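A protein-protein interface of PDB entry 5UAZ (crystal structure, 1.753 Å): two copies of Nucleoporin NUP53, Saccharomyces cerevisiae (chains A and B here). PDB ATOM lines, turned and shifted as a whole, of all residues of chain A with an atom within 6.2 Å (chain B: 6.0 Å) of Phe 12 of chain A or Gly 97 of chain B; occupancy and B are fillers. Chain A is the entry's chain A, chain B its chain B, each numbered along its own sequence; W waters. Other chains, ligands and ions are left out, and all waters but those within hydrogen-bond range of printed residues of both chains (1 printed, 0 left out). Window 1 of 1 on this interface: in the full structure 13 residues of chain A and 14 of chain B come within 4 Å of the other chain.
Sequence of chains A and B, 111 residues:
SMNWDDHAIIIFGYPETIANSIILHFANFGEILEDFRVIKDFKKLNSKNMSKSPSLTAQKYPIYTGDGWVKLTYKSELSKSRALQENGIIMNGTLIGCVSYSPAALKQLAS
The side-chain amide oxygen (OD1) of Asn 87 of chain B sits at hydrogen-bond distance from the side-chain amide nitrogen (ND2) of Asn 87 of chain A (3.1 Å).
O of Ile 89 of chain B lies within hydrogen-bond range of N of Ile 96 of chain B, 2.9 Å away. O of Phe 12 of chain A sits at hydrogen-bond distance from N of Gly 97 of chain A (2.8 Å). N of Ile 10 of chain B is in hydrogen-bond range of O of Val 99 of chain B (2.8 Å). N of Ile 10 of chain A is in hydrogen-bond range of O of Val 99 of chain A (2.8 Å). The backbone NH of Gly 88 of chain B lies within hydrogen-bond range of the backbone carbonyl oxygen of Ile 96 of chain B, 2.7 Å away. The backbone carbonyl oxygen of Phe 12 of chain B sits at hydrogen-bond distance from the backbone NH of Gly 97 of chain B.
Ile 10 of chain A touches Leu 95 of chain B (CG2 to CD1, 3.5 Å). Phe 12 of chain A touches Leu 95 of chain B (CD1 to O, 3.6 Å). Phe 12 of chain A touches Ile 96 of chain B (CE1 to C, 3.9 Å). Gly 97 of chain B touches Phe 12 of chain A (N to CE1, 3.7 Å). Asn 87 of chain A touches Val 99 of chain B. CD1 of Leu 95 of chain A touches CG2 of Ile 10 of chain B, at 3.6 Å. Leu 95 of chain A touches Phe 12 of chain B. CE2 of Phe 12 of chain B touches C of Ile 96 of chain A, 3.7 Å away. Phe 12 of chain B touches Gly 97 of chain A (CE2 to N, 3.6 Å). CA of Gly 88 of chain B touches CG1 of Val 99 of chain A (3.8 Å).
Phe 12 of chain A touches three residues of chain B. Of the printed residues of chain B, Asn 87 of chain A touches Phe 12, Asn 87 and Val 99. Printed residues of chain B within 4 Å of Leu 95 of chain A: Ile 10 and Phe 12. Printed residues of chain A within 4 Å of Leu 95 of chain B: Ile 10 and Phe 12. The nearest residue of chain A that does not touch Gly 97 of chain B is Asn 87 of chain A (5.0 Å). The nearest printed residue of chain A that does not touch Gly 88 of chain B is Phe 12 of chain A (5.1 Å).
Of the 14 printed residues of chain A, 7 touch a printed residue of chain B. Printed residues of chain A that touch a printed residue of chain B: Ile 10, Phe 12, Asn 87, Leu 95, Ile 96, Gly 97 and Val 99. Hydrophobic or aromatic side chains of chain A that line the printed part of chain B: Ile 10, Phe 12, Leu 95 and Val 99. Of the 14 printed residues of chain B, 8 touch a printed residue of chain A. Hydrophobic or aromatic side chains of chain B that line the printed part of chain A: Ile 10, Phe 12, Leu 95 and Val 99. Among the printed residues, no Asp or Glu carboxylate lies within 4 Å of a Lys or Arg side-chain nitrogen of the other chain.
Phe 12 of chain A touches Leu 95 of chain B, and with the chains exchanged Leu 95 of chain A touches Phe 12 of chain B. Phe 12 of chain A touches Ile 96 of chain B, and with the chains exchanged Ile 96 of chain A touches Phe 12 of chain B. Phe 12 of chain A touches Gly 97 of chain B, and with the chains exchanged Gly 97 of chain A touches Phe 12 of chain B. Asn 87 of chain A touches Val 99 of chain B, and with the chains exchanged Val 99 of chain A touches Asn 87 of chain B. Positions printed for both chains: 10, 11, 12, 13, 87, 95, 96, 97, 98 and 99.
Water W1 lies within hydrogen-bond range of the backbone carbonyl oxygen of Cys 98 of chain A (2.7 Å) and the side-chain amide nitrogen of Asn 87 of chain B (3.1 Å).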
ATOM      1  N   ILE A  10      -4.366  17.395 -28.483  1.00  0.00           N
ATOM      2  CA  ILE A  10      -3.737  16.082 -28.639  1.00  0.00           C
ATOM      3  C   ILE A  10      -3.758  15.411 -27.274  1.00  0.00           C
ATOM      4  O   ILE A  10      -3.322  15.992 -26.262  1.00  0.00           O
ATOM      5  CB  ILE A  10      -2.274  16.175 -29.158  1.00  0.00           C
ATOM      6  CG1 ILE A  10      -2.215  16.963 -30.458  1.00  0.00           C
ATOM      7  CG2 ILE A  10      -1.708  14.777 -29.274  1.00  0.00           C
ATOM      8  CD1 ILE A  10      -0.820  17.337 -30.987  1.00  0.00           C
ATOM      9  N   ILE A  11      -4.279  14.206 -27.228  1.00  0.00           N
ATOM     10  CA  ILE A  11      -4.308  13.434 -26.007  1.00  0.00           C
ATOM     11  C   ILE A  11      -3.216  12.392 -26.158  1.00  0.00           C
ATOM     12  O   ILE A  11      -3.101  11.808 -27.238  1.00  0.00           O
ATOM     13  CB  ILE A  11      -5.672  12.770 -25.792  1.00  0.00           C
ATOM     14  CG1 ILE A  11      -6.752  13.845 -25.754  1.00  0.00           C
ATOM     15  CG2 ILE A  11      -5.693  12.043 -24.464  1.00  0.00           C
ATOM     16  CD1 ILE A  11      -8.039  13.310 -26.223  1.00  0.00           C
ATOM     17  N   PHE A  12      -2.501  12.078 -25.088  1.00  0.00           N
ATOM     18  CA  PHE A  12      -1.336  11.231 -25.276  1.00  0.00           C
ATOM     19  C   PHE A  12      -0.995  10.453 -24.010  1.00  0.00           C
ATOM     20  O   PHE A  12      -1.494  10.710 -22.912  1.00  0.00           O
ATOM     21  CB  PHE A  12      -0.121  12.069 -25.733  1.00  0.00           C
ATOM     22  CG  PHE A  12       0.330  13.079 -24.751  1.00  0.00           C
ATOM     23  CD1 PHE A  12       1.243  12.753 -23.786  1.00  0.00           C
ATOM     24  CD2 PHE A  12      -0.189  14.374 -24.790  1.00  0.00           C
ATOM     25  CE1 PHE A  12       1.672  13.715 -22.872  1.00  0.00           C
ATOM     26  CE2 PHE A  12       0.199  15.314 -23.915  1.00  0.00           C
ATOM     27  CZ  PHE A  12       1.166  15.002 -22.947  1.00  0.00           C
ATOM     28  N   GLY A  13      -0.124   9.467 -24.193  1.00  0.00           N
ATOM     29  CA  GLY A  13       0.487   8.829 -23.064  1.00  0.00           C
ATOM     30  C   GLY A  13      -0.134   7.532 -22.632  1.00  0.00           C
ATOM     31  O   GLY A  13       0.366   6.898 -21.673  1.00  0.00           O
ATOM     32  N   TYR A  14      -1.162   7.069 -23.345  1.00  0.00           N
ATOM     33  CA  TYR A  14      -1.926   5.943 -22.876  1.00  0.00           C
ATOM     34  C   TYR A  14      -1.540   4.687 -23.640  1.00  0.00           C
ATOM     35  O   TYR A  14      -1.070   4.767 -24.773  1.00  0.00           O
ATOM     36  CB  TYR A  14      -3.419   6.239 -23.065  1.00  0.00           C
ATOM     37  CG  TYR A  14      -3.793   6.689 -24.458  1.00  0.00           C
ATOM     38  CD1 TYR A  14      -4.066   5.770 -25.459  1.00  0.00           C
ATOM     39  CD2 TYR A  14      -3.897   8.043 -24.800  1.00  0.00           C
ATOM     40  CE1 TYR A  14      -4.402   6.190 -26.736  1.00  0.00           C
ATOM     41  CE2 TYR A  14      -4.235   8.438 -26.062  1.00  0.00           C
ATOM     42  CZ  TYR A  14      -4.478   7.530 -27.017  1.00  0.00           C
ATOM     43  OH  TYR A  14      -4.860   7.940 -28.281  1.00  0.00           O
ATOM     44  N   GLY A  68      -0.658   5.481 -28.827  1.00  0.00           N
ATOM     45  CA  GLY A  68      -0.591   6.262 -27.625  1.00  0.00           C
ATOM     46  C   GLY A  68      -0.945   7.723 -27.766  1.00  0.00           C
ATOM     47  O   GLY A  68      -0.739   8.466 -26.801  1.00  0.00           O
ATOM     48  N   TRP A  69      -1.489   8.159 -28.904  1.00  0.00           N
ATOM     49  CA  TRP A  69      -1.927   9.549 -29.004  1.00  0.00           C
ATOM     50  C   TRP A  69      -3.008   9.698 -30.068  1.00  0.00           C
ATOM     51  O   TRP A  69      -3.139   8.901 -31.031  1.00  0.00           O
ATOM     52  CB  TRP A  69      -0.757  10.508 -29.336  1.00  0.00           C
ATOM     53  CG  TRP A  69      -0.097  10.248 -30.676  1.00  0.00           C
ATOM     54  CD1 TRP A  69       0.984   9.392 -30.908  1.00  0.00           C
ATOM     55  CD2 TRP A  69      -0.427  10.818 -31.958  1.00  0.00           C
ATOM     56  NE1 TRP A  69       1.338   9.426 -32.242  1.00  0.00           N
ATOM     57  CE2 TRP A  69       0.460  10.254 -32.918  1.00  0.00           C
ATOM     58  CE3 TRP A  69      -1.400  11.730 -32.404  1.00  0.00           C
ATOM     59  CZ2 TRP A  69       0.409  10.601 -34.236  1.00  0.00           C
ATOM     60  CZ3 TRP A  69      -1.445  12.055 -33.734  1.00  0.00           C
ATOM     61  CH2 TRP A  69      -0.556  11.487 -34.637  1.00  0.00           C
ATOM     62  N   VAL A  70      -3.777  10.767 -29.886  1.00  0.00           N
ATOM     63  CA  VAL A  70      -4.814  11.111 -30.853  1.00  0.00           C
ATOM     64  C   VAL A  70      -5.055  12.622 -30.838  1.00  0.00           C
ATOM     65  O   VAL A  70      -5.034  13.257 -29.775  1.00  0.00           O
ATOM     66  CB  VAL A  70      -6.129  10.361 -30.554  1.00  0.00           C
ATOM     67  CG1 VAL A  70      -6.738  10.781 -29.267  1.00  0.00           C
ATOM     68  CG2 VAL A  70      -7.117  10.512 -31.718  1.00  0.00           C
ATOM     69  N   ASN A  87      -5.321  17.332 -18.342  1.00  0.00           N
ATOM     70  CA  ASN A  87      -3.905  16.950 -18.350  1.00  0.00           C
ATOM     71  C   ASN A  87      -3.460  16.410 -16.976  1.00  0.00           C
ATOM     72  O   ASN A  87      -3.536  17.100 -15.958  1.00  0.00           O
ATOM     73  CB  ASN A  87      -3.061  18.153 -18.783  1.00  0.00           C
ATOM     74  CG  ASN A  87      -1.604  17.741 -19.196  1.00  0.00           C
ATOM     75  OD1 ASN A  87      -1.372  16.708 -19.837  1.00  0.00           O
ATOM     76  ND2 ASN A  87      -0.645  18.564 -18.825  1.00  0.00           N
ATOM     77  N   LEU A  95      -1.164   7.857 -16.251  1.00  0.00           N
ATOM     78  CA  LEU A  95      -1.318   9.301 -16.432  1.00  0.00           C
ATOM     79  C   LEU A  95      -1.608   9.604 -17.883  1.00  0.00           C
ATOM     80  O   LEU A  95      -0.904   9.109 -18.772  1.00  0.00           O
ATOM     81  CB  LEU A  95      -0.036  10.046 -16.020  1.00  0.00           C
ATOM     82  CG  LEU A  95       0.124  10.133 -14.521  1.00  0.00           C
ATOM     83  CD1 LEU A  95       1.621  10.209 -14.123  1.00  0.00           C
ATOM     84  CD2 LEU A  95      -0.661  11.362 -14.028  1.00  0.00           C
ATOM     85  N   ILE A  96      -2.633  10.442 -18.117  1.00  0.00           N
ATOM     86  CA  ILE A  96      -3.086  10.826 -19.438  1.00  0.00           C
ATOM     87  C   ILE A  96      -2.698  12.278 -19.690  1.00  0.00           C
ATOM     88  O   ILE A  96      -2.932  13.145 -18.839  1.00  0.00           O
ATOM     89  CB  ILE A  96      -4.609  10.665 -19.581  1.00  0.00           C
ATOM     90  CG1 ILE A  96      -5.065   9.292 -19.042  1.00  0.00           C
ATOM     91  CG2 ILE A  96      -5.000  10.964 -20.947  1.00  0.00           C
ATOM     92  CD1 ILE A  96      -4.463   8.134 -19.786  1.00  0.00           C
ATOM     93  N   GLY A  97      -2.064  12.539 -20.835  1.00  0.00           N
ATOM     94  CA  GLY A  97      -1.661  13.890 -21.191  1.00  0.00           C
ATOM     95  C   GLY A  97      -2.682  14.496 -22.150  1.00  0.00           C
ATOM     96  O   GLY A  97      -3.296  13.785 -22.930  1.00  0.00           O
ATOM     97  N   CYS A  98      -2.886  15.822 -22.037  1.00  0.00           N
ATOM     98  CA  CYS A  98      -3.813  16.577 -22.885  1.00  0.00           C
ATOM     99  C   CYS A  98      -3.136  17.916 -23.111  1.00  0.00           C
ATOM    100  O   CYS A  98      -2.900  18.648 -22.150  1.00  0.00           O
ATOM    101  CB  CYS A  98      -5.201  16.756 -22.233  1.00  0.00           C
ATOM    102  SG  CYS A  98      -6.250  17.581 -23.455  1.00  0.00           S
ATOM    103  N   VAL A  99      -2.765  18.230 -24.356  1.00  0.00           N
ATOM    104  CA  VAL A  99      -2.236  19.543 -24.674  1.00  0.00           C
ATOM    105  C   VAL A  99      -2.997  20.126 -25.842  1.00  0.00           C
ATOM    106  O   VAL A  99      -3.631  19.422 -26.621  1.00  0.00           O
ATOM    107  CB  VAL A  99      -0.741  19.536 -25.015  1.00  0.00           C
ATOM    108  CG1 VAL A  99       0.105  19.144 -23.779  1.00  0.00           C
ATOM    109  CG2 VAL A  99      -0.434  18.622 -26.229  1.00  0.00           C
ATOM    110  N   ILE B  10       5.284  15.897 -11.631  1.00  0.00           N
ATOM    111  CA  ILE B  10       5.288  14.565 -12.206  1.00  0.00           C
ATOM    112  C   ILE B  10       5.495  14.726 -13.700  1.00  0.00           C
ATOM    113  O   ILE B  10       4.826  15.554 -14.345  1.00  0.00           O
ATOM    114  CB  ILE B  10       3.982  13.803 -11.894  1.00  0.00           C
ATOM    115  CG1 ILE B  10       3.846  13.546 -10.401  1.00  0.00           C
ATOM    116  CG2 ILE B  10       3.984  12.422 -12.520  1.00  0.00           C
ATOM    117  CD1 ILE B  10       2.450  13.101  -9.996  1.00  0.00           C
ATOM    118  N   ILE B  11       6.451  13.974 -14.231  1.00  0.00           N
ATOM    119  CA  ILE B  11       6.741  13.929 -15.657  1.00  0.00           C
ATOM    120  C   ILE B  11       6.298  12.564 -16.126  1.00  0.00           C
ATOM    121  O   ILE B  11       6.495  11.560 -15.424  1.00  0.00           O
ATOM    122  CB  ILE B  11       8.229  14.161 -15.944  1.00  0.00           C
ATOM    123  CG1 ILE B  11       8.675  15.445 -15.267  1.00  0.00           C
ATOM    124  CG2 ILE B  11       8.501  14.278 -17.443  1.00  0.00           C
ATOM    125  CD1 ILE B  11      10.160  15.292 -14.831  1.00  0.00           C
ATOM    126  N   PHE B  12       5.640  12.529 -17.285  1.00  0.00           N
ATOM    127  CA  PHE B  12       5.077  11.267 -17.744  1.00  0.00           C
ATOM    128  C   PHE B  12       4.944  11.207 -19.233  1.00  0.00           C
ATOM    129  O   PHE B  12       5.011  12.211 -19.946  1.00  0.00           O
ATOM    130  CB  PHE B  12       3.693  11.030 -17.117  1.00  0.00           C
ATOM    131  CG  PHE B  12       2.671  12.080 -17.489  1.00  0.00           C
ATOM    132  CD1 PHE B  12       2.534  13.219 -16.739  1.00  0.00           C
ATOM    133  CD2 PHE B  12       1.861  11.936 -18.576  1.00  0.00           C
ATOM    134  CE1 PHE B  12       1.559  14.182 -17.069  1.00  0.00           C
ATOM    135  CE2 PHE B  12       0.929  12.881 -18.955  1.00  0.00           C
ATOM    136  CZ  PHE B  12       0.744  14.010 -18.191  1.00  0.00           C
ATOM    137  N   GLY B  13       4.793   9.975 -19.712  1.00  0.00           N
ATOM    138  CA  GLY B  13       4.440   9.724 -21.092  1.00  0.00           C
ATOM    139  C   GLY B  13       5.570   9.226 -21.972  1.00  0.00           C
ATOM    140  O   GLY B  13       5.322   8.897 -23.143  1.00  0.00           O
ATOM    141  N   PHE B  26      15.264  17.504 -16.936  1.00  0.00           N
ATOM    142  CA  PHE B  26      14.525  18.314 -15.969  1.00  0.00           C
ATOM    143  C   PHE B  26      15.381  18.731 -14.791  1.00  0.00           C
ATOM    144  O   PHE B  26      15.141  19.799 -14.167  1.00  0.00           O
ATOM    145  CB  PHE B  26      13.248  17.551 -15.528  1.00  0.00           C
ATOM    146  CG  PHE B  26      12.123  17.654 -16.540  1.00  0.00           C
ATOM    147  CD1 PHE B  26      11.980  16.760 -17.632  1.00  0.00           C
ATOM    148  CD2 PHE B  26      11.198  18.694 -16.399  1.00  0.00           C
ATOM    149  CE1 PHE B  26      10.947  16.924 -18.535  1.00  0.00           C
ATOM    150  CE2 PHE B  26      10.163  18.872 -17.313  1.00  0.00           C
ATOM    151  CZ  PHE B  26      10.015  17.961 -18.366  1.00  0.00           C
ATOM    152  N   GLU B  86       7.752  22.988 -19.776  1.00  0.00           N
ATOM    153  CA  GLU B  86       8.092  21.925 -20.712  1.00  0.00           C
ATOM    154  C   GLU B  86       6.930  21.001 -21.028  1.00  0.00           C
ATOM    155  O   GLU B  86       7.079  20.135 -21.901  1.00  0.00           O
ATOM    156  CB  GLU B  86       9.223  21.080 -20.138  1.00  0.00           C
ATOM    157  CG  GLU B  86      10.518  21.830 -19.945  1.00  0.00           C
ATOM    158  CD  GLU B  86      11.091  22.397 -21.244  1.00  0.00           C
ATOM    159  OE1 GLU B  86      11.801  21.645 -21.960  1.00  0.00           O
ATOM    160  OE2 GLU B  86      10.841  23.596 -21.541  1.00  0.00           O
ATOM    161  N   ASN B  87       5.786  21.149 -20.359  1.00  0.00           N
ATOM    162  CA  ASN B  87       4.640  20.330 -20.688  1.00  0.00           C
ATOM    163  C   ASN B  87       4.343  20.407 -22.168  1.00  0.00           C
ATOM    164  O   ASN B  87       4.173  21.488 -22.719  1.00  0.00           O
ATOM    165  CB  ASN B  87       3.427  20.785 -19.878  1.00  0.00           C
ATOM    166  CG  ASN B  87       2.230  19.981 -20.085  1.00  0.00           C
ATOM    167  OD1 ASN B  87       2.209  18.791 -19.896  1.00  0.00           O
ATOM    168  ND2 ASN B  87       1.129  20.663 -20.430  1.00  0.00           N
ATOM    169  N   GLY B  88       4.237  19.251 -22.788  1.00  0.00           N
ATOM    170  CA  GLY B  88       3.917  19.117 -24.179  1.00  0.00           C
ATOM    171  C   GLY B  88       5.093  19.132 -25.154  1.00  0.00           C
ATOM    172  O   GLY B  88       4.843  19.077 -26.367  1.00  0.00           O
ATOM    173  N   ILE B  89       6.341  19.203 -24.687  1.00  0.00           N
ATOM    174  CA  ILE B  89       7.488  19.041 -25.633  1.00  0.00           C
ATOM    175  C   ILE B  89       7.493  17.613 -26.129  1.00  0.00           C
ATOM    176  O   ILE B  89       6.866  16.734 -25.550  1.00  0.00           O
ATOM    177  CB  ILE B  89       8.855  19.383 -25.033  1.00  0.00           C
ATOM    178  CG1 ILE B  89       9.148  18.487 -23.861  1.00  0.00           C
ATOM    179  CG2 ILE B  89       8.875  20.858 -24.597  1.00  0.00           C
ATOM    180  CD1 ILE B  89      10.606  18.509 -23.437  1.00  0.00           C
ATOM    181  N   LEU B  95       5.188  12.743 -27.061  1.00  0.00           N
ATOM    182  CA  LEU B  95       4.826  13.856 -26.197  1.00  0.00           C
ATOM    183  C   LEU B  95       5.110  13.563 -24.722  1.00  0.00           C
ATOM    184  O   LEU B  95       4.794  12.468 -24.201  1.00  0.00           O
ATOM    185  CB  LEU B  95       3.331  14.182 -26.399  1.00  0.00           C
ATOM    186  CG  LEU B  95       3.008  15.059 -27.613  1.00  0.00           C
ATOM    187  CD1 LEU B  95       1.487  14.989 -27.931  1.00  0.00           C
ATOM    188  CD2 LEU B  95       3.415  16.506 -27.438  1.00  0.00           C
ATOM    189  N   ILE B  96       5.603  14.615 -24.025  1.00  0.00           N
ATOM    190  CA  ILE B  96       5.968  14.588 -22.580  1.00  0.00           C
ATOM    191  C   ILE B  96       5.016  15.468 -21.794  1.00  0.00           C
ATOM    192  O   ILE B  96       4.841  16.652 -22.125  1.00  0.00           O
ATOM    193  CB  ILE B  96       7.405  15.077 -22.350  1.00  0.00           C
ATOM    194  CG1 ILE B  96       8.379  14.391 -23.291  1.00  0.00           C
ATOM    195  CG2 ILE B  96       7.809  14.834 -20.885  1.00  0.00           C
ATOM    196  CD1 ILE B  96       8.462  12.881 -23.066  1.00  0.00           C
ATOM    197  N   GLY B  97       4.401  14.899 -20.752  1.00  0.00           N
ATOM    198  CA  GLY B  97       3.515  15.633 -19.880  1.00  0.00           C
ATOM    199  C   GLY B  97       4.300  16.093 -18.668  1.00  0.00           C
ATOM    200  O   GLY B  97       5.230  15.414 -18.220  1.00  0.00           O
ATOM    201  N   CYS B  98       3.983  17.287 -18.164  1.00  0.00           N
ATOM    202  CA  CYS B  98       4.632  17.721 -16.913  1.00  0.00           C
ATOM    203  C   CYS B  98       3.551  18.447 -16.140  1.00  0.00           C
ATOM    204  O   CYS B  98       3.080  19.487 -16.607  1.00  0.00           O
ATOM    205  CB  CYS B  98       5.834  18.628 -17.182  1.00  0.00           C
ATOM    206  SG  CYS B  98       6.709  19.124 -15.659  1.00  0.00           S
ATOM    207  N   VAL B  99       3.134  17.896 -14.984  1.00  0.00           N
ATOM    208  CA  VAL B  99       2.117  18.526 -14.157  1.00  0.00           C
ATOM    209  C   VAL B  99       2.605  18.712 -12.731  1.00  0.00           C
ATOM    210  O   VAL B  99       3.504  18.023 -12.226  1.00  0.00           O
ATOM    211  CB  VAL B  99       0.826  17.721 -14.149  1.00  0.00           C
ATOM    212  CG1 VAL B  99       0.189  17.707 -15.578  1.00  0.00           C
ATOM    213  CG2 VAL B  99       1.044  16.284 -13.592  1.00  0.00           C
HETATM  214  O   HOH W   1      -1.845  20.967 -21.302  1.00  0.00           O
